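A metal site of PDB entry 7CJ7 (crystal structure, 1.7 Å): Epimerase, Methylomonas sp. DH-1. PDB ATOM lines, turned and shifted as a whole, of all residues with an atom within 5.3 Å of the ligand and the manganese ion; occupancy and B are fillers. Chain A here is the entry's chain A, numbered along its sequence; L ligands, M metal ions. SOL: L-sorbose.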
ATOM      1  N   HIS A  12     -17.723 -26.288  21.026  1.00  0.00           N
ATOM      2  CA  HIS A  12     -17.244 -26.190  22.428  1.00  0.00           C
ATOM      3  C   HIS A  12     -18.166 -27.027  23.308  1.00  0.00           C
ATOM      4  O   HIS A  12     -19.385 -27.011  23.075  1.00  0.00           O
ATOM      5  CB  HIS A  12     -17.188 -24.719  22.840  1.00  0.00           C
ATOM      6  CG  HIS A  12     -16.486 -24.507  24.133  1.00  0.00           C
ATOM      7  ND1 HIS A  12     -17.155 -24.530  25.330  1.00  0.00           N
ATOM      8  CD2 HIS A  12     -15.189 -24.246  24.412  1.00  0.00           C
ATOM      9  CE1 HIS A  12     -16.300 -24.304  26.307  1.00  0.00           C
ATOM     10  NE2 HIS A  12     -15.094 -24.118  25.769  1.00  0.00           N
ATOM     11  N   GLU A  41     -14.461 -29.545  21.293  1.00  0.00           N
ATOM     12  CA  GLU A  41     -13.420 -28.837  22.060  1.00  0.00           C
ATOM     13  C   GLU A  41     -13.737 -29.035  23.535  1.00  0.00           C
ATOM     14  O   GLU A  41     -14.762 -28.517  23.993  1.00  0.00           O
ATOM     15  CB  GLU A  41     -13.365 -27.358  21.672  1.00  0.00           C
ATOM     16  CG  GLU A  41     -12.194 -26.645  22.304  1.00  0.00           C
ATOM     17  CD  GLU A  41     -12.156 -25.193  21.897  1.00  0.00           C
ATOM     18  OE1 GLU A  41     -11.999 -24.923  20.689  1.00  0.00           O
ATOM     19  OE2 GLU A  41     -12.347 -24.336  22.791  1.00  0.00           O
ATOM     20  N   ALA A  43     -13.248 -28.462  27.436  1.00  0.00           N
ATOM     21  CA  ALA A  43     -12.785 -27.462  28.415  1.00  0.00           C
ATOM     22  C   ALA A  43     -12.046 -28.195  29.540  1.00  0.00           C
ATOM     23  O   ALA A  43     -12.684 -28.982  30.229  1.00  0.00           O
ATOM     24  CB  ALA A  43     -13.968 -26.675  28.918  1.00  0.00           C
ATOM     25  N   LEU A  45     -10.277 -26.994  32.329  1.00  0.00           N
ATOM     26  CA  LEU A  45      -9.926 -26.086  33.453  1.00  0.00           C
ATOM     27  C   LEU A  45      -9.345 -26.907  34.614  1.00  0.00           C
ATOM     28  O   LEU A  45      -8.418 -26.400  35.287  1.00  0.00           O
ATOM     29  CB  LEU A  45     -11.162 -25.287  33.848  1.00  0.00           C
ATOM     30  CG  LEU A  45     -11.339 -23.969  33.099  1.00  0.00           C
ATOM     31  CD1 LEU A  45     -11.673 -24.205  31.631  1.00  0.00           C
ATOM     32  CD2 LEU A  45     -12.410 -23.123  33.757  1.00  0.00           C
ATOM     33  N   SER A  69      -9.247 -26.759  25.173  1.00  0.00           N
ATOM     34  CA  SER A  69      -9.013 -25.352  25.568  1.00  0.00           C
ATOM     35  C   SER A  69      -9.054 -25.284  27.091  1.00  0.00           C
ATOM     36  O   SER A  69      -9.684 -26.165  27.709  1.00  0.00           O
ATOM     37  CB  SER A  69     -10.019 -24.433  24.913  1.00  0.00           C
ATOM     38  OG  SER A  69     -11.321 -24.693  25.395  1.00  0.00           O
ATOM     39  N   LEU A  70      -8.393 -24.297  27.672  1.00  0.00           N
ATOM     40  CA  LEU A  70      -8.576 -24.020  29.109  1.00  0.00           C
ATOM     41  C   LEU A  70      -8.234 -22.563  29.380  1.00  0.00           C
ATOM     42  O   LEU A  70      -7.723 -21.884  28.497  1.00  0.00           O
ATOM     43  CB  LEU A  70      -7.704 -24.972  29.920  1.00  0.00           C
ATOM     44  CG  LEU A  70      -6.201 -24.840  29.681  1.00  0.00           C
ATOM     45  CD1 LEU A  70      -5.607 -23.722  30.524  1.00  0.00           C
ATOM     46  CD2 LEU A  70      -5.499 -26.154  29.959  1.00  0.00           C
ATOM     47  N   GLY A  71      -8.619 -22.108  30.564  1.00  0.00           N
ATOM     48  CA  GLY A  71      -8.100 -20.890  31.189  1.00  0.00           C
ATOM     49  C   GLY A  71      -7.430 -21.250  32.496  1.00  0.00           C
ATOM     50  O   GLY A  71      -7.922 -22.176  33.159  1.00  0.00           O
ATOM     51  N   CYS A 109      -5.539 -24.912  23.160  1.00  0.00           N
ATOM     52  CA  CYS A 109      -5.837 -23.497  22.856  1.00  0.00           C
ATOM     53  C   CYS A 109      -6.546 -22.825  24.032  1.00  0.00           C
ATOM     54  O   CYS A 109      -6.694 -23.454  25.101  1.00  0.00           O
ATOM     55  CB  CYS A 109      -6.637 -23.391  21.556  1.00  0.00           C
ATOM     56  SG  CYS A 109      -8.332 -24.014  21.684  1.00  0.00           S
ATOM     57  N   GLY A 110      -6.899 -21.560  23.880  1.00  0.00           N
ATOM     58  CA  GLY A 110      -7.564 -20.787  24.933  1.00  0.00           C
ATOM     59  C   GLY A 110      -6.602 -19.899  25.703  1.00  0.00           C
ATOM     60  O   GLY A 110      -5.510 -19.549  25.189  1.00  0.00           O
ATOM     61  N   VAL A 111      -7.008 -19.512  26.898  1.00  0.00           N
ATOM     62  CA  VAL A 111      -6.255 -18.548  27.736  1.00  0.00           C
ATOM     63  C   VAL A 111      -5.263 -19.343  28.581  1.00  0.00           C
ATOM     64  O   VAL A 111      -5.488 -19.526  29.792  1.00  0.00           O
ATOM     65  CB  VAL A 111      -7.223 -17.663  28.550  1.00  0.00           C
ATOM     66  CG1 VAL A 111      -6.463 -16.643  29.387  1.00  0.00           C
ATOM     67  CG2 VAL A 111      -8.201 -16.970  27.625  1.00  0.00           C
ATOM     68  N   LEU A 116      -7.605 -16.656  33.465  1.00  0.00           N
ATOM     69  CA  LEU A 116      -8.819 -16.204  32.729  1.00  0.00           C
ATOM     70  C   LEU A 116      -9.679 -15.430  33.730  1.00  0.00           C
ATOM     71  O   LEU A 116     -10.093 -16.049  34.730  1.00  0.00           O
ATOM     72  CB  LEU A 116      -9.564 -17.423  32.183  1.00  0.00           C
ATOM     73  CG  LEU A 116     -10.859 -17.111  31.431  1.00  0.00           C
ATOM     74  CD1 LEU A 116     -10.575 -16.308  30.186  1.00  0.00           C
ATOM     75  CD2 LEU A 116     -11.597 -18.394  31.074  1.00  0.00           C
ATOM     76  N   GLU A 152      -5.124 -17.721  22.855  1.00  0.00           N
ATOM     77  CA  GLU A 152      -6.385 -17.025  22.541  1.00  0.00           C
ATOM     78  C   GLU A 152      -6.314 -15.583  23.053  1.00  0.00           C
ATOM     79  O   GLU A 152      -6.236 -15.376  24.270  1.00  0.00           O
ATOM     80  CB  GLU A 152      -7.583 -17.753  23.141  1.00  0.00           C
ATOM     81  CG  GLU A 152      -8.890 -17.238  22.579  1.00  0.00           C
ATOM     82  CD  GLU A 152     -10.101 -17.950  23.139  1.00  0.00           C
ATOM     83  OE1 GLU A 152      -9.935 -18.774  24.096  1.00  0.00           O
ATOM     84  OE2 GLU A 152     -11.187 -17.697  22.629  1.00  0.00           O
ATOM     85  N   VAL A 154      -8.120 -12.452  24.171  1.00  0.00           N
ATOM     86  CA  VAL A 154      -9.463 -12.251  24.752  1.00  0.00           C
ATOM     87  C   VAL A 154      -9.579 -10.802  25.201  1.00  0.00           C
ATOM     88  O   VAL A 154      -8.558 -10.076  25.219  1.00  0.00           O
ATOM     89  CB  VAL A 154      -9.765 -13.231  25.899  1.00  0.00           C
ATOM     90  CG1 VAL A 154      -9.828 -14.666  25.397  1.00  0.00           C
ATOM     91  CG2 VAL A 154      -8.763 -13.084  27.030  1.00  0.00           C
ATOM     92  N   GLU A 158     -11.064 -10.215  30.550  1.00  0.00           N
ATOM     93  CA  GLU A 158     -10.683 -11.648  30.662  1.00  0.00           C
ATOM     94  C   GLU A 158      -9.153 -11.845  30.663  1.00  0.00           C
ATOM     95  O   GLU A 158      -8.720 -12.940  31.061  1.00  0.00           O
ATOM     96  CB  GLU A 158     -11.372 -12.466  29.561  1.00  0.00           C
ATOM     97  CG  GLU A 158     -12.892 -12.532  29.720  1.00  0.00           C
ATOM     98  CD  GLU A 158     -13.579 -13.505  28.780  1.00  0.00           C
ATOM     99  OE1 GLU A 158     -12.889 -14.439  28.316  1.00  0.00           O
ATOM    100  OE2 GLU A 158     -14.778 -13.307  28.475  1.00  0.00           O
ATOM    101  N   HIS A 183      -4.608 -17.465  18.401  1.00  0.00           N
ATOM    102  CA  HIS A 183      -5.993 -17.969  18.416  1.00  0.00           C
ATOM    103  C   HIS A 183      -6.908 -16.756  18.477  1.00  0.00           C
ATOM    104  O   HIS A 183      -6.740 -15.949  19.408  1.00  0.00           O
ATOM    105  CB  HIS A 183      -6.120 -18.977  19.566  1.00  0.00           C
ATOM    106  CG  HIS A 183      -7.502 -19.435  19.892  1.00  0.00           C
ATOM    107  ND1 HIS A 183      -7.740 -20.274  20.965  1.00  0.00           N
ATOM    108  CD2 HIS A 183      -8.706 -19.183  19.317  1.00  0.00           C
ATOM    109  CE1 HIS A 183      -9.041 -20.509  21.047  1.00  0.00           C
ATOM    110  NE2 HIS A 183      -9.651 -19.868  20.047  1.00  0.00           N
ATOM    111  N   ASP A 185     -10.900 -15.055  18.334  1.00  0.00           N
ATOM    112  CA  ASP A 185     -12.290 -15.370  18.740  1.00  0.00           C
ATOM    113  C   ASP A 185     -13.157 -14.158  18.378  1.00  0.00           C
ATOM    114  O   ASP A 185     -12.885 -13.068  18.894  1.00  0.00           O
ATOM    115  CB  ASP A 185     -12.317 -15.710  20.233  1.00  0.00           C
ATOM    116  CG  ASP A 185     -13.696 -16.031  20.778  1.00  0.00           C
ATOM    117  OD1 ASP A 185     -14.660 -15.429  20.323  1.00  0.00           O
ATOM    118  OD2 ASP A 185     -13.772 -16.891  21.655  1.00  0.00           O
ATOM    119  N   TYR A 187     -16.022 -13.097  19.155  1.00  0.00           N
ATOM    120  CA  TYR A 187     -16.681 -12.424  20.299  1.00  0.00           C
ATOM    121  C   TYR A 187     -15.721 -11.380  20.898  1.00  0.00           C
ATOM    122  O   TYR A 187     -16.130 -10.232  21.149  1.00  0.00           O
ATOM    123  CB  TYR A 187     -17.118 -13.431  21.361  1.00  0.00           C
ATOM    124  CG  TYR A 187     -17.428 -12.820  22.701  1.00  0.00           C
ATOM    125  CD1 TYR A 187     -18.596 -12.116  22.924  1.00  0.00           C
ATOM    126  CD2 TYR A 187     -16.539 -12.938  23.758  1.00  0.00           C
ATOM    127  CE1 TYR A 187     -18.872 -11.538  24.153  1.00  0.00           C
ATOM    128  CE2 TYR A 187     -16.809 -12.368  24.987  1.00  0.00           C
ATOM    129  CZ  TYR A 187     -17.995 -11.691  25.201  1.00  0.00           C
ATOM    130  OH  TYR A 187     -18.266 -11.121  26.410  1.00  0.00           O
ATOM    131  N   HIS A 188     -14.477 -11.783  21.142  1.00  0.00           N
ATOM    132  CA  HIS A 188     -13.443 -10.897  21.729  1.00  0.00           C
ATOM    133  C   HIS A 188     -13.030  -9.809  20.727  1.00  0.00           C
ATOM    134  O   HIS A 188     -12.834  -8.661  21.145  1.00  0.00           O
ATOM    135  CB  HIS A 188     -12.269 -11.731  22.237  1.00  0.00           C
ATOM    136  CG  HIS A 188     -12.674 -12.663  23.337  1.00  0.00           C
ATOM    137  ND1 HIS A 188     -13.091 -12.197  24.562  1.00  0.00           N
ATOM    138  CD2 HIS A 188     -12.719 -14.010  23.394  1.00  0.00           C
ATOM    139  CE1 HIS A 188     -13.378 -13.231  25.338  1.00  0.00           C
ATOM    140  NE2 HIS A 188     -13.147 -14.354  24.643  1.00  0.00           N
ATOM    141  N   HIS A 211     -12.187 -19.277  17.090  1.00  0.00           N
ATOM    142  CA  HIS A 211     -13.528 -19.368  17.723  1.00  0.00           C
ATOM    143  C   HIS A 211     -14.506 -18.439  17.007  1.00  0.00           C
ATOM    144  O   HIS A 211     -14.179 -17.247  16.799  1.00  0.00           O
ATOM    145  CB  HIS A 211     -13.477 -19.062  19.211  1.00  0.00           C
ATOM    146  CG  HIS A 211     -12.948 -20.194  20.016  1.00  0.00           C
ATOM    147  ND1 HIS A 211     -12.791 -20.094  21.380  1.00  0.00           N
ATOM    148  CD2 HIS A 211     -12.531 -21.422  19.664  1.00  0.00           C
ATOM    149  CE1 HIS A 211     -12.362 -21.245  21.849  1.00  0.00           C
ATOM    150  NE2 HIS A 211     -12.159 -22.076  20.813  1.00  0.00           N
ATOM    151  N   ARG A 217     -22.707 -13.949  22.560  1.00  0.00           N
ATOM    152  CA  ARG A 217     -22.315 -15.376  22.751  1.00  0.00           C
ATOM    153  C   ARG A 217     -23.529 -16.301  22.591  1.00  0.00           C
ATOM    154  O   ARG A 217     -23.445 -17.468  23.053  1.00  0.00           O
ATOM    155  CB  ARG A 217     -21.640 -15.595  24.117  1.00  0.00           C
ATOM    156  CG  ARG A 217     -20.628 -14.530  24.513  1.00  0.00           C
ATOM    157  CD  ARG A 217     -19.558 -15.012  25.495  1.00  0.00           C
ATOM    158  NE  ARG A 217     -18.436 -15.665  24.823  1.00  0.00           N
ATOM    159  CZ  ARG A 217     -17.234 -15.854  25.348  1.00  0.00           C
ATOM    160  NH1 ARG A 217     -16.980 -15.496  26.588  1.00  0.00           N
ATOM    161  NH2 ARG A 217     -16.296 -16.421  24.633  1.00  0.00           N
ATOM    162  N   GLU A 246     -18.565 -21.442  19.598  1.00  0.00           N
ATOM    163  CA  GLU A 246     -18.540 -21.219  21.057  1.00  0.00           C
ATOM    164  C   GLU A 246     -19.765 -20.385  21.441  1.00  0.00           C
ATOM    165  O   GLU A 246     -20.030 -19.355  20.797  1.00  0.00           O
ATOM    166  CB  GLU A 246     -17.232 -20.545  21.454  1.00  0.00           C
ATOM    167  CG  GLU A 246     -17.086 -20.393  22.949  1.00  0.00           C
ATOM    168  CD  GLU A 246     -15.665 -20.089  23.373  1.00  0.00           C
ATOM    169  OE1 GLU A 246     -15.082 -20.886  24.144  1.00  0.00           O
ATOM    170  OE2 GLU A 246     -15.142 -19.081  22.898  1.00  0.00           O
ATOM    171  N   PHE A 248     -22.464 -19.525  25.135  1.00  0.00           N
ATOM    172  CA  PHE A 248     -22.774 -19.718  26.569  1.00  0.00           C
ATOM    173  C   PHE A 248     -24.168 -19.193  26.861  1.00  0.00           C
ATOM    174  O   PHE A 248     -24.521 -18.072  26.420  1.00  0.00           O
ATOM    175  CB  PHE A 248     -21.707 -19.055  27.436  1.00  0.00           C
ATOM    176  CG  PHE A 248     -20.308 -19.551  27.183  1.00  0.00           C
ATOM    177  CD1 PHE A 248     -19.848 -20.719  27.781  1.00  0.00           C
ATOM    178  CD2 PHE A 248     -19.451 -18.856  26.347  1.00  0.00           C
ATOM    179  CE1 PHE A 248     -18.558 -21.175  27.522  1.00  0.00           C
ATOM    180  CE2 PHE A 248     -18.175 -19.310  26.099  1.00  0.00           C
ATOM    181  CZ  PHE A 248     -17.736 -20.468  26.687  1.00  0.00           C
ATOM    182  N   LEU A 257     -16.344 -21.772  35.115  1.00  0.00           N
ATOM    183  CA  LEU A 257     -16.162 -21.036  33.834  1.00  0.00           C
ATOM    184  C   LEU A 257     -17.328 -20.051  33.625  1.00  0.00           C
ATOM    185  O   LEU A 257     -17.057 -18.912  33.229  1.00  0.00           O
ATOM    186  CB  LEU A 257     -16.068 -22.026  32.673  1.00  0.00           C
ATOM    187  CG  LEU A 257     -15.765 -21.433  31.288  1.00  0.00           C
ATOM    188  CD1 LEU A 257     -14.465 -20.641  31.305  1.00  0.00           C
ATOM    189  CD2 LEU A 257     -15.722 -22.516  30.210  1.00  0.00           C
ATOM    190  N   LEU A 261     -17.049 -15.965  33.137  1.00  0.00           N
ATOM    191  CA  LEU A 261     -17.442 -15.374  31.829  1.00  0.00           C
ATOM    192  C   LEU A 261     -18.711 -14.530  31.975  1.00  0.00           C
ATOM    193  O   LEU A 261     -19.191 -13.990  30.960  1.00  0.00           O
ATOM    194  CB  LEU A 261     -17.651 -16.490  30.791  1.00  0.00           C
ATOM    195  CG  LEU A 261     -16.409 -17.325  30.476  1.00  0.00           C
ATOM    196  CD1 LEU A 261     -16.681 -18.271  29.309  1.00  0.00           C
ATOM    197  CD2 LEU A 261     -15.222 -16.423  30.166  1.00  0.00           C
HETATM  198  C1  SOL L   1     -13.323 -17.276  26.954  1.00  0.00           C
HETATM  199  O1  SOL L   1     -14.046 -16.072  26.847  1.00  0.00           O
HETATM  200  C2  SOL L   1     -13.223 -17.976  25.632  1.00  0.00           C
HETATM  201  O2  SOL L   1     -13.367 -17.362  24.594  1.00  0.00           O
HETATM  202  C3  SOL L   1     -12.982 -19.479  25.628  1.00  0.00           C
HETATM  203  O3  SOL L   1     -12.482 -19.905  24.390  1.00  0.00           O
HETATM  204  C4  SOL L   1     -12.048 -19.894  26.755  1.00  0.00           C
HETATM  205  O4  SOL L   1     -10.775 -19.257  26.573  1.00  0.00           O
HETATM  206  C5  SOL L   1     -11.820 -21.409  26.842  1.00  0.00           C
HETATM  207  O5  SOL L   1     -10.790 -21.680  27.794  1.00  0.00           O
HETATM  208  C6  SOL L   1     -13.067 -22.182  27.224  1.00  0.00           C
HETATM  209  O6  SOL L   1     -12.800 -23.589  27.239  1.00  0.00           O
HETATM  210 MN    MN M   1     -13.123 -18.433  22.767  1.00  0.00          MN
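OD2 of Asp 185 lies close to NH2 of Arg 217, at 3.9 Å. OD1 of Asp 185 is in hydrogen-bond range of N of Tyr 187, at 2.9 Å. OE2 of Glu 246 lies close to NH2 of Arg 217 (3.4 Å). NE2 of His 211 lies within hydrogen-bond range of OE1 of Glu 41, 2.9 Å away. The side-chain carboxylate (OE2) of Glu 158 is in salt-bridge range of the guanidinium group (NH1) of Arg 217 (3.6 Å). The backbone carbonyl oxygen (O) of Arg 217 sits at hydrogen-bond distance from the backbone NH (N) of Phe 248, at 3.1 Å. The backbone NH (N) of Leu 70 sits at hydrogen-bond distance from the backbone carbonyl oxygen (O) of Cys 109 (3.2 Å). N of Gly 110 sits at hydrogen-bond distance from ND1 of His 183 (3.3 Å).
OD2 of Asp 185 is bound to the manganese ion. The side-chain carboxylate (OE2) of Glu 152 binds the manganese ion, at 2.1 Å. The side-chain carboxylate (OE2) of Glu 246 is bound to the manganese ion (2.1 Å). O2 of the ligand is bound to the manganese ion, at 2.1 Å. ND1 of His 211 binds the manganese ion, 2.2 Å away. The manganese ion is bound by O3 of the ligand (2.3 Å).
The side-chain carboxylate of Glu 158 is in hydrogen-bond range of an oxygen (O1) of the ligand (2.5 Å). OG of Ser 69 sits at hydrogen-bond distance from O6 of the ligand (2.6 Å). NE2 of His 12 is in hydrogen-bond range of O6 of the ligand (2.8 Å). O1 of the ligand sits at hydrogen-bond distance from NE2 of His 188, at 2.9 Å. The guanidinium group of Arg 217 sits at hydrogen-bond distance from an oxygen (O1) of the ligand, 3.0 Å away. O of Leu 70 sits close to O5 of the ligand.
Residues that only touch the ligand: Leu 261 (3.5 Å), Gly 71 (3.5 Å), Val 111 (3.6 Å), Ala 43 (3.7 Å) and Gly 110 (3.9 Å). Hydrophobic or aromatic side chains within 4 Å of the ligand: His 12, Ala 43, Val 111, His 188, His 211 and Leu 261. Within 4 Å of the ligand: His 12, Ala 43, Ser 69, Leu 70, Gly 71, Gly 110, Val 111, Glu 152, Glu 158, Asp 185, His 188, His 211, Arg 217, Glu 246 and Leu 261. The nearest printed residue that does not touch the ligand is Leu 257 (4.01 Å).
Four residues have an atom within 4 Å of the manganese ion: Glu 152, Asp 185, His 211 and Glu 246.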
